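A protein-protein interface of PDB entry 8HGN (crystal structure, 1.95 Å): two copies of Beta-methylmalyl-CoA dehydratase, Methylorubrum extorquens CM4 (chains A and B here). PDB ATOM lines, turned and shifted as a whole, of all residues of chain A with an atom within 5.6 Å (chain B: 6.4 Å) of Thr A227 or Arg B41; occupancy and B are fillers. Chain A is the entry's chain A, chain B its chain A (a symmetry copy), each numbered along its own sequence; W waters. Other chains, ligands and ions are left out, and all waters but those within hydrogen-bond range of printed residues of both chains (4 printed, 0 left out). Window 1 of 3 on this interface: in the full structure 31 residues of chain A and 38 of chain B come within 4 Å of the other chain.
Among the printed residues, pairs that only touch across the chains: Thr A22 with Thr B43 (3.3 Å), Thr A22 with Ser B46 (3.6 Å), Thr A22 with Phe B261 (3.8 Å), Pro A76 with Arg B41 (3.9 Å), Leu A80 with Asp B208 (3.96 Å), Gln A225 with Arg B41 (3.9 Å), Thr A227 with Arg B41 (3.1 Å) and Lys A229 with Asp B208 (3.6 Å).
Water W3 lies within hydrogen-bond range of O of Thr A227 (2.7 Å) and OD1 of Asp B208 (3.4 Å). Water W2 bridges the side-chain hydroxyl (OG1) of Thr A22 and the guanidinium group (NH2) of Arg B41. Water W4 lies within hydrogen-bond range of the side-chain carboxylate of Asp B208, the side-chain amino group of Lys A229 and the side-chain amide nitrogen of Asn B262. Water W1 bridges the side-chain hydroxyl (OG1) of Thr A227 and the guanidinium group (NH2) of Arg B41.
Of the 14 printed residues of chain A, 6 touch a printed residue of chain B. Printed residues of chain A that touch a printed residue of chain B: Thr A22, Pro A76, Leu A80, Gln A225, Thr A227 and Lys A229. Hydrophobic or aromatic side chains of chain A that line the printed part of chain B: Pro A76 and Leu A80. Along chain A the printed residues that touch a printed residue of chain B span positions 22 to 229. Of the 15 printed residues of chain B, 7 touch a printed residue of chain A. Hydrophobic or aromatic side chains of chain B that line the printed part of chain A: Phe B261. Among the printed residues, 12 pairs touch across the chains.
The backbone carbonyl oxygen (O) of Pro B40 lies within hydrogen-bond range of the side-chain amide nitrogen (NE2) of Gln A225, 3.0 Å away. The side-chain hydroxyl (OG1) of Thr A22 is in hydrogen-bond range of the backbone carbonyl oxygen (O) of Arg B41 (2.7 Å). The backbone NH of Thr A22 lies within hydrogen-bond range of the backbone carbonyl oxygen of Leu B188 (2.8 Å). NE2 of Gln A225 lies within hydrogen-bond range of OG of Ser B46 (3.2 Å).
No position is printed for both chains.
Of the printed residues of chain B, Leu A80 touches Asp B208 (3.96 Å). Of the printed residues of chain B, Gln A225 touches Pro B40, Arg B41 and Ser B46. Of the printed residues of chain B, Thr A227 touches Arg B41. Printed residues of chain B within 4 Å of Lys A229: Asp B208. Val A230 touches none of the printed residues of chain B. Of chain A, only Thr A22, Pro A76, Gln A225 and Thr A227 come within 4 Å of Arg B41. Leu B259 touches none of the printed residues of chain A. Of the printed residues of chain A, Phe B261 touches Thr A22. The nearest residue of chain B that does not touch Thr A227 is Asp B208 (5.1 Å). The nearest printed residue of chain A that does not touch Arg B41 is Asn A226 (5.8 Å).
The backbone carbonyl oxygen (O) of Val A75 is in hydrogen-bond range of the backbone NH (N) of Leu A80. O of Leu A80 is in hydrogen-bond range of N of Lys A229 (3.2 Å). OG1 of Thr B43 sits at hydrogen-bond distance from O of Leu B188 (2.9 Å).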
ATOM      1  N   THR A  22      -6.656  33.589  -7.377  1.00  0.00           N
ATOM      2  CA  THR A  22      -6.950  33.290  -5.948  1.00  0.00           C
ATOM      3  C   THR A  22      -7.146  34.588  -5.178  1.00  0.00           C
ATOM      4  O   THR A  22      -6.307  34.954  -4.359  1.00  0.00           O
ATOM      5  CB  THR A  22      -5.874  32.395  -5.313  1.00  0.00           C
ATOM      6  OG1 THR A  22      -5.606  31.276  -6.170  1.00  0.00           O
ATOM      7  CG2 THR A  22      -6.285  31.905  -3.937  1.00  0.00           C
ATOM      8  N   GLY A  72       0.993  38.459  -1.796  1.00  0.00           N
ATOM      9  CA  GLY A  72       0.860  36.991  -1.872  1.00  0.00           C
ATOM     10  C   GLY A  72       0.289  36.544  -3.198  1.00  0.00           C
ATOM     11  O   GLY A  72       0.914  35.747  -3.881  1.00  0.00           O
ATOM     12  N   VAL A  75       2.442  36.379  -6.152  1.00  0.00           N
ATOM     13  CA  VAL A  75       3.703  35.583  -6.145  1.00  0.00           C
ATOM     14  C   VAL A  75       3.644  34.490  -7.220  1.00  0.00           C
ATOM     15  O   VAL A  75       4.578  34.371  -7.992  1.00  0.00           O
ATOM     16  CB  VAL A  75       4.113  35.114  -4.742  1.00  0.00           C
ATOM     17  CG1 VAL A  75       5.251  34.115  -4.793  1.00  0.00           C
ATOM     18  CG2 VAL A  75       4.500  36.317  -3.873  1.00  0.00           C
ATOM     19  N   PRO A  76       2.579  33.674  -7.360  1.00  0.00           N
ATOM     20  CA  PRO A  76       2.561  32.615  -8.378  1.00  0.00           C
ATOM     21  C   PRO A  76       3.067  33.033  -9.777  1.00  0.00           C
ATOM     22  O   PRO A  76       3.794  32.272 -10.407  1.00  0.00           O
ATOM     23  CB  PRO A  76       1.080  32.249  -8.433  1.00  0.00           C
ATOM     24  CG  PRO A  76       0.591  32.472  -7.012  1.00  0.00           C
ATOM     25  CD  PRO A  76       1.349  33.699  -6.551  1.00  0.00           C
ATOM     26  N   LEU A  80       7.382  33.257  -8.044  1.00  0.00           N
ATOM     27  CA  LEU A  80       7.362  31.817  -7.680  1.00  0.00           C
ATOM     28  C   LEU A  80       8.787  31.293  -7.749  1.00  0.00           C
ATOM     29  O   LEU A  80       9.159  30.470  -6.876  1.00  0.00           O
ATOM     30  CB  LEU A  80       6.459  31.085  -8.670  1.00  0.00           C
ATOM     31  CG  LEU A  80       6.510  29.566  -8.618  1.00  0.00           C
ATOM     32  CD1 LEU A  80       6.177  29.051  -7.221  1.00  0.00           C
ATOM     33  CD2 LEU A  80       5.549  28.988  -9.648  1.00  0.00           C
ATOM     34  N   THR A 221       3.856  32.413   5.552  1.00  0.00           N
ATOM     35  CA  THR A 221       4.053  32.594   4.108  1.00  0.00           C
ATOM     36  C   THR A 221       2.893  31.911   3.409  1.00  0.00           C
ATOM     37  O   THR A 221       2.342  32.541   2.504  1.00  0.00           O
ATOM     38  CB  THR A 221       5.417  32.109   3.596  1.00  0.00           C
ATOM     39  OG1 THR A 221       6.395  32.807   4.378  1.00  0.00           O
ATOM     40  CG2 THR A 221       5.564  32.400   2.113  1.00  0.00           C
ATOM     41  N   GLN A 225      -0.651  32.936   1.054  1.00  0.00           N
ATOM     42  CA  GLN A 225      -0.738  32.117  -0.188  1.00  0.00           C
ATOM     43  C   GLN A 225       0.392  32.541  -1.153  1.00  0.00           C
ATOM     44  O   GLN A 225       0.152  32.649  -2.394  1.00  0.00           O
ATOM     45  CB  GLN A 225      -2.129  32.276  -0.810  1.00  0.00           C
ATOM     46  CG  GLN A 225      -3.189  31.447  -0.130  1.00  0.00           C
ATOM     47  CD  GLN A 225      -4.590  31.914  -0.435  1.00  0.00           C
ATOM     48  OE1 GLN A 225      -4.852  33.122  -0.541  1.00  0.00           O
ATOM     49  NE2 GLN A 225      -5.490  30.950  -0.589  1.00  0.00           N
ATOM     50  N   ASN A 226       1.530  32.901  -0.584  1.00  0.00           N
ATOM     51  CA  ASN A 226       2.813  33.265  -1.261  1.00  0.00           C
ATOM     52  C   ASN A 226       3.563  31.944  -1.466  1.00  0.00           C
ATOM     53  O   ASN A 226       3.750  31.209  -0.462  1.00  0.00           O
ATOM     54  CB  ASN A 226       3.572  34.283  -0.402  1.00  0.00           C
ATOM     55  CG  ASN A 226       5.039  34.475  -0.710  1.00  0.00           C
ATOM     56  OD1 ASN A 226       5.713  33.641  -1.332  1.00  0.00           O
ATOM     57  ND2 ASN A 226       5.565  35.588  -0.250  1.00  0.00           N
ATOM     58  N   THR A 227       3.887  31.607  -2.710  1.00  0.00           N
ATOM     59  CA  THR A 227       4.310  30.241  -3.119  1.00  0.00           C
ATOM     60  C   THR A 227       5.818  30.168  -3.393  1.00  0.00           C
ATOM     61  O   THR A 227       6.254  29.078  -3.789  1.00  0.00           O
ATOM     62  CB  THR A 227       3.465  29.785  -4.306  1.00  0.00           C
ATOM     63  OG1 THR A 227       3.580  30.858  -5.232  1.00  0.00           O
ATOM     64  CG2 THR A 227       2.001  29.566  -3.985  1.00  0.00           C
ATOM     65  N   ALA A 228       6.605  31.220  -3.145  1.00  0.00           N
ATOM     66  CA  ALA A 228       8.006  31.290  -3.634  1.00  0.00           C
ATOM     67  C   ALA A 228       8.769  30.079  -3.091  1.00  0.00           C
ATOM     68  O   ALA A 228       8.903  30.008  -1.860  1.00  0.00           O
ATOM     69  CB  ALA A 228       8.696  32.561  -3.220  1.00  0.00           C
ATOM     70  N   LYS A 229       9.234  29.193  -3.985  1.00  0.00           N
ATOM     71  CA  LYS A 229       9.746  27.827  -3.662  1.00  0.00           C
ATOM     72  C   LYS A 229      10.871  27.918  -2.621  1.00  0.00           C
ATOM     73  O   LYS A 229      10.945  27.051  -1.727  1.00  0.00           O
ATOM     74  CB  LYS A 229      10.251  27.145  -4.942  1.00  0.00           C
ATOM     75  CG  LYS A 229       9.200  26.764  -5.966  1.00  0.00           C
ATOM     76  CD  LYS A 229       9.755  26.750  -7.381  1.00  0.00           C
ATOM     77  CE  LYS A 229       9.181  25.669  -8.252  1.00  0.00           C
ATOM     78  NZ  LYS A 229       8.981  26.176  -9.625  1.00  0.00           N
ATOM     79  N   VAL A 230      11.667  28.974  -2.666  1.00  0.00           N
ATOM     80  CA  VAL A 230      12.831  29.207  -1.760  1.00  0.00           C
ATOM     81  C   VAL A 230      12.400  29.302  -0.273  1.00  0.00           C
ATOM     82  O   VAL A 230      13.246  29.050   0.631  1.00  0.00           O
ATOM     83  CB  VAL A 230      13.606  30.438  -2.273  1.00  0.00           C
ATOM     84  CG1 VAL A 230      14.004  31.423  -1.196  1.00  0.00           C
ATOM     85  CG2 VAL A 230      14.819  30.041  -3.093  1.00  0.00           C
ATOM     86  N   HIS A 231      11.118  29.549   0.013  1.00  0.00           N
ATOM     87  CA  HIS A 231      10.583  29.559   1.407  1.00  0.00           C
ATOM     88  C   HIS A 231      10.390  28.138   1.952  1.00  0.00           C
ATOM     89  O   HIS A 231      10.481  27.935   3.174  1.00  0.00           O
ATOM     90  CB  HIS A 231       9.299  30.391   1.460  1.00  0.00           C
ATOM     91  CG  HIS A 231       9.505  31.787   1.013  1.00  0.00           C
ATOM     92  ND1 HIS A 231      10.637  32.508   1.342  1.00  0.00           N
ATOM     93  CD2 HIS A 231       8.785  32.579   0.189  1.00  0.00           C
ATOM     94  CE1 HIS A 231      10.572  33.718   0.784  1.00  0.00           C
ATOM     95  NE2 HIS A 231       9.435  33.789   0.087  1.00  0.00           N
ATOM     96  N   PHE A 232      10.155  27.170   1.074  1.00  0.00           N
ATOM     97  CA  PHE A 232       9.470  25.938   1.469  1.00  0.00           C
ATOM     98  C   PHE A 232      10.285  24.662   1.237  1.00  0.00           C
ATOM     99  O   PHE A 232       9.902  23.645   1.865  1.00  0.00           O
ATOM    100  CB  PHE A 232       8.152  25.875   0.710  1.00  0.00           C
ATOM    101  CG  PHE A 232       7.179  26.939   1.131  1.00  0.00           C
ATOM    102  CD1 PHE A 232       6.826  27.064   2.457  1.00  0.00           C
ATOM    103  CD2 PHE A 232       6.723  27.880   0.213  1.00  0.00           C
ATOM    104  CE1 PHE A 232       5.922  28.051   2.843  1.00  0.00           C
ATOM    105  CE2 PHE A 232       5.825  28.858   0.610  1.00  0.00           C
ATOM    106  CZ  PHE A 232       5.430  28.942   1.910  1.00  0.00           C
ATOM    107  N   GLY B  39      -1.616  25.721   2.558  1.00  0.00           N
ATOM    108  CA  GLY B  39      -1.460  26.702   1.468  1.00  0.00           C
ATOM    109  C   GLY B  39      -2.351  26.461   0.253  1.00  0.00           C
ATOM    110  O   GLY B  39      -1.981  26.881  -0.841  1.00  0.00           O
ATOM    111  N   PRO B  40      -3.573  25.884   0.360  1.00  0.00           N
ATOM    112  CA  PRO B  40      -4.404  25.665  -0.824  1.00  0.00           C
ATOM    113  C   PRO B  40      -4.875  27.000  -1.421  1.00  0.00           C
ATOM    114  O   PRO B  40      -4.997  27.967  -0.709  1.00  0.00           O
ATOM    115  CB  PRO B  40      -5.574  24.854  -0.269  1.00  0.00           C
ATOM    116  CG  PRO B  40      -5.727  25.419   1.095  1.00  0.00           C
ATOM    117  CD  PRO B  40      -4.298  25.548   1.589  1.00  0.00           C
ATOM    118  N   ARG B  41      -5.011  27.050  -2.742  1.00  0.00           N
ATOM    119  CA  ARG B  41      -5.266  28.319  -3.466  1.00  0.00           C
ATOM    120  C   ARG B  41      -6.503  28.173  -4.348  1.00  0.00           C
ATOM    121  O   ARG B  41      -6.696  29.022  -5.199  1.00  0.00           O
ATOM    122  CB  ARG B  41      -4.019  28.687  -4.273  1.00  0.00           C
ATOM    123  CG  ARG B  41      -2.908  29.279  -3.428  1.00  0.00           C
ATOM    124  CD  ARG B  41      -1.712  29.713  -4.247  1.00  0.00           C
ATOM    125  NE  ARG B  41      -0.903  28.561  -4.585  1.00  0.00           N
ATOM    126  CZ  ARG B  41      -0.547  28.179  -5.785  1.00  0.00           C
ATOM    127  NH1 ARG B  41       0.196  27.084  -5.893  1.00  0.00           N
ATOM    128  NH2 ARG B  41      -0.892  28.885  -6.862  1.00  0.00           N
ATOM    129  N   PHE B  42      -7.309  27.133  -4.135  1.00  0.00           N
ATOM    130  CA  PHE B  42      -8.605  26.936  -4.827  1.00  0.00           C
ATOM    131  C   PHE B  42      -9.536  28.076  -4.425  1.00  0.00           C
ATOM    132  O   PHE B  42      -9.886  28.229  -3.218  1.00  0.00           O
ATOM    133  CB  PHE B  42      -9.215  25.589  -4.456  1.00  0.00           C
ATOM    134  CG  PHE B  42      -8.358  24.409  -4.815  1.00  0.00           C
ATOM    135  CD1 PHE B  42      -8.338  23.912  -6.121  1.00  0.00           C
ATOM    136  CD2 PHE B  42      -7.642  23.750  -3.842  1.00  0.00           C
ATOM    137  CE1 PHE B  42      -7.554  22.826  -6.447  1.00  0.00           C
ATOM    138  CE2 PHE B  42      -6.879  22.647  -4.173  1.00  0.00           C
ATOM    139  CZ  PHE B  42      -6.823  22.198  -5.473  1.00  0.00           C
ATOM    140  N   THR B  43      -9.962  28.846  -5.427  1.00  0.00           N
ATOM    141  CA  THR B  43     -10.671  30.142  -5.235  1.00  0.00           C
ATOM    142  C   THR B  43     -12.053  29.920  -4.621  1.00  0.00           C
ATOM    143  O   THR B  43     -12.467  30.715  -3.729  1.00  0.00           O
ATOM    144  CB  THR B  43     -10.611  30.884  -6.576  1.00  0.00           C
ATOM    145  OG1 THR B  43      -9.215  31.012  -6.881  1.00  0.00           O
ATOM    146  CG2 THR B  43     -11.297  32.226  -6.542  1.00  0.00           C
ATOM    147  N   VAL B  44     -12.768  28.860  -4.997  1.00  0.00           N
ATOM    148  CA  VAL B  44     -14.113  28.618  -4.396  1.00  0.00           C
ATOM    149  C   VAL B  44     -13.990  28.721  -2.869  1.00  0.00           C
ATOM    150  O   VAL B  44     -14.823  29.385  -2.265  1.00  0.00           O
ATOM    151  CB  VAL B  44     -14.751  27.289  -4.834  1.00  0.00           C
ATOM    152  CG1 VAL B  44     -15.896  26.922  -3.934  1.00  0.00           C
ATOM    153  CG2 VAL B  44     -15.197  27.329  -6.287  1.00  0.00           C
ATOM    154  N   SER B  46     -11.345  29.945  -1.018  1.00  0.00           N
ATOM    155  CA  SER B  46     -10.521  31.108  -0.598  1.00  0.00           C
ATOM    156  C   SER B  46     -11.304  32.430  -0.662  1.00  0.00           C
ATOM    157  O   SER B  46     -11.058  33.272   0.233  1.00  0.00           O
ATOM    158  CB  SER B  46      -9.275  31.174  -1.449  1.00  0.00           C
ATOM    159  OG  SER B  46      -8.401  32.213  -1.012  1.00  0.00           O
ATOM    160  N   LEU B 188      -9.570  34.577 -12.028  1.00  0.00           N
ATOM    161  CA  LEU B 188      -9.685  34.511 -10.549  1.00  0.00           C
ATOM    162  C   LEU B 188      -9.510  33.061 -10.075  1.00  0.00           C
ATOM    163  O   LEU B 188      -8.806  32.888  -9.108  1.00  0.00           O
ATOM    164  CB  LEU B 188     -11.022  35.114 -10.108  1.00  0.00           C
ATOM    165  CG  LEU B 188     -11.180  36.612 -10.402  1.00  0.00           C
ATOM    166  CD1 LEU B 188     -12.386  37.183  -9.669  1.00  0.00           C
ATOM    167  CD2 LEU B 188      -9.913  37.389 -10.045  1.00  0.00           C
ATOM    168  N   ALA B 189     -10.049  32.044 -10.759  1.00  0.00           N
ATOM    169  CA  ALA B 189      -9.844  30.619 -10.393  1.00  0.00           C
ATOM    170  C   ALA B 189      -8.411  30.106 -10.727  1.00  0.00           C
ATOM    171  O   ALA B 189      -7.998  29.151 -10.072  1.00  0.00           O
ATOM    172  CB  ALA B 189     -10.921  29.757 -11.022  1.00  0.00           C
ATOM    173  N   ASP B 208       5.988  21.740  -7.348  1.00  0.00           N
ATOM    174  CA  ASP B 208       6.245  22.429  -6.052  1.00  0.00           C
ATOM    175  C   ASP B 208       6.556  21.398  -4.952  1.00  0.00           C
ATOM    176  O   ASP B 208       5.934  20.352  -4.934  1.00  0.00           O
ATOM    177  CB  ASP B 208       5.045  23.302  -5.650  1.00  0.00           C
ATOM    178  CG  ASP B 208       4.833  24.470  -6.601  1.00  0.00           C
ATOM    179  OD1 ASP B 208       5.837  25.115  -6.956  1.00  0.00           O
ATOM    180  OD2 ASP B 208       3.705  24.656  -7.045  1.00  0.00           O
ATOM    181  N   ALA B 258      -3.175  20.393  -2.040  1.00  0.00           N
ATOM    182  CA  ALA B 258      -2.735  21.801  -2.227  1.00  0.00           C
ATOM    183  C   ALA B 258      -1.820  21.876  -3.447  1.00  0.00           C
ATOM    184  O   ALA B 258      -2.139  22.635  -4.392  1.00  0.00           O
ATOM    185  CB  ALA B 258      -2.084  22.368  -1.000  1.00  0.00           C
ATOM    186  N   LEU B 259      -0.743  21.087  -3.481  1.00  0.00           N
ATOM    187  CA  LEU B 259       0.231  21.108  -4.611  1.00  0.00           C
ATOM    188  C   LEU B 259      -0.537  20.936  -5.931  1.00  0.00           C
ATOM    189  O   LEU B 259      -0.252  21.680  -6.861  1.00  0.00           O
ATOM    190  CB  LEU B 259       1.263  19.995  -4.361  1.00  0.00           C
ATOM    191  CG  LEU B 259       2.097  20.179  -3.090  1.00  0.00           C
ATOM    192  CD1 LEU B 259       3.045  18.994  -2.880  1.00  0.00           C
ATOM    193  CD2 LEU B 259       2.900  21.471  -3.163  1.00  0.00           C
ATOM    194  N   PHE B 261      -3.219  21.946  -7.051  1.00  0.00           N
ATOM    195  CA  PHE B 261      -3.691  23.246  -7.601  1.00  0.00           C
ATOM    196  C   PHE B 261      -2.847  23.605  -8.824  1.00  0.00           C
ATOM    197  O   PHE B 261      -3.341  24.319  -9.707  1.00  0.00           O
ATOM    198  CB  PHE B 261      -3.602  24.346  -6.538  1.00  0.00           C
ATOM    199  CG  PHE B 261      -4.081  25.690  -7.026  1.00  0.00           C
ATOM    200  CD1 PHE B 261      -3.203  26.586  -7.600  1.00  0.00           C
ATOM    201  CD2 PHE B 261      -5.423  25.979  -7.045  1.00  0.00           C
ATOM    202  CE1 PHE B 261      -3.659  27.789  -8.107  1.00  0.00           C
ATOM    203  CE2 PHE B 261      -5.889  27.182  -7.562  1.00  0.00           C
ATOM    204  CZ  PHE B 261      -4.995  28.095  -8.061  1.00  0.00           C
ATOM    205  N   ASN B 262      -1.583  23.179  -8.849  1.00  0.00           N
ATOM    206  CA  ASN B 262      -0.692  23.411 -10.013  1.00  0.00           C
ATOM    207  C   ASN B 262      -1.069  22.388 -11.093  1.00  0.00           C
ATOM    208  O   ASN B 262      -0.402  21.330 -11.137  1.00  0.00           O
ATOM    209  CB  ASN B 262       0.791  23.411  -9.614  1.00  0.00           C
ATOM    210  CG  ASN B 262       1.683  24.025 -10.676  1.00  0.00           C
ATOM    211  OD1 ASN B 262       1.200  24.571 -11.668  1.00  0.00           O
ATOM    212  ND2 ASN B 262       2.994  23.940 -10.491  1.00  0.00           N
ATOM    213  N   ALA B 265      -6.555  23.450 -10.800  1.00  0.00           N
ATOM    214  CA  ALA B 265      -7.121  24.606 -10.059  1.00  0.00           C
ATOM    215  C   ALA B 265      -8.649  24.612 -10.144  1.00  0.00           C
ATOM    216  O   ALA B 265      -9.295  25.050  -9.147  1.00  0.00           O
ATOM    217  CB  ALA B 265      -6.546  25.882 -10.595  1.00  0.00           C
HETATM  218  O   HOH W   1       2.433  29.353  -7.505  1.00  0.00           O
HETATM  219  O   HOH W   2      -2.909  31.466  -7.177  1.00  0.00           O
HETATM  220  O   HOH W   3       5.831  26.390  -3.791  1.00  0.00           O
HETATM  221  O   HOH W   4       5.880  25.345  -9.880  1.00  0.00           O
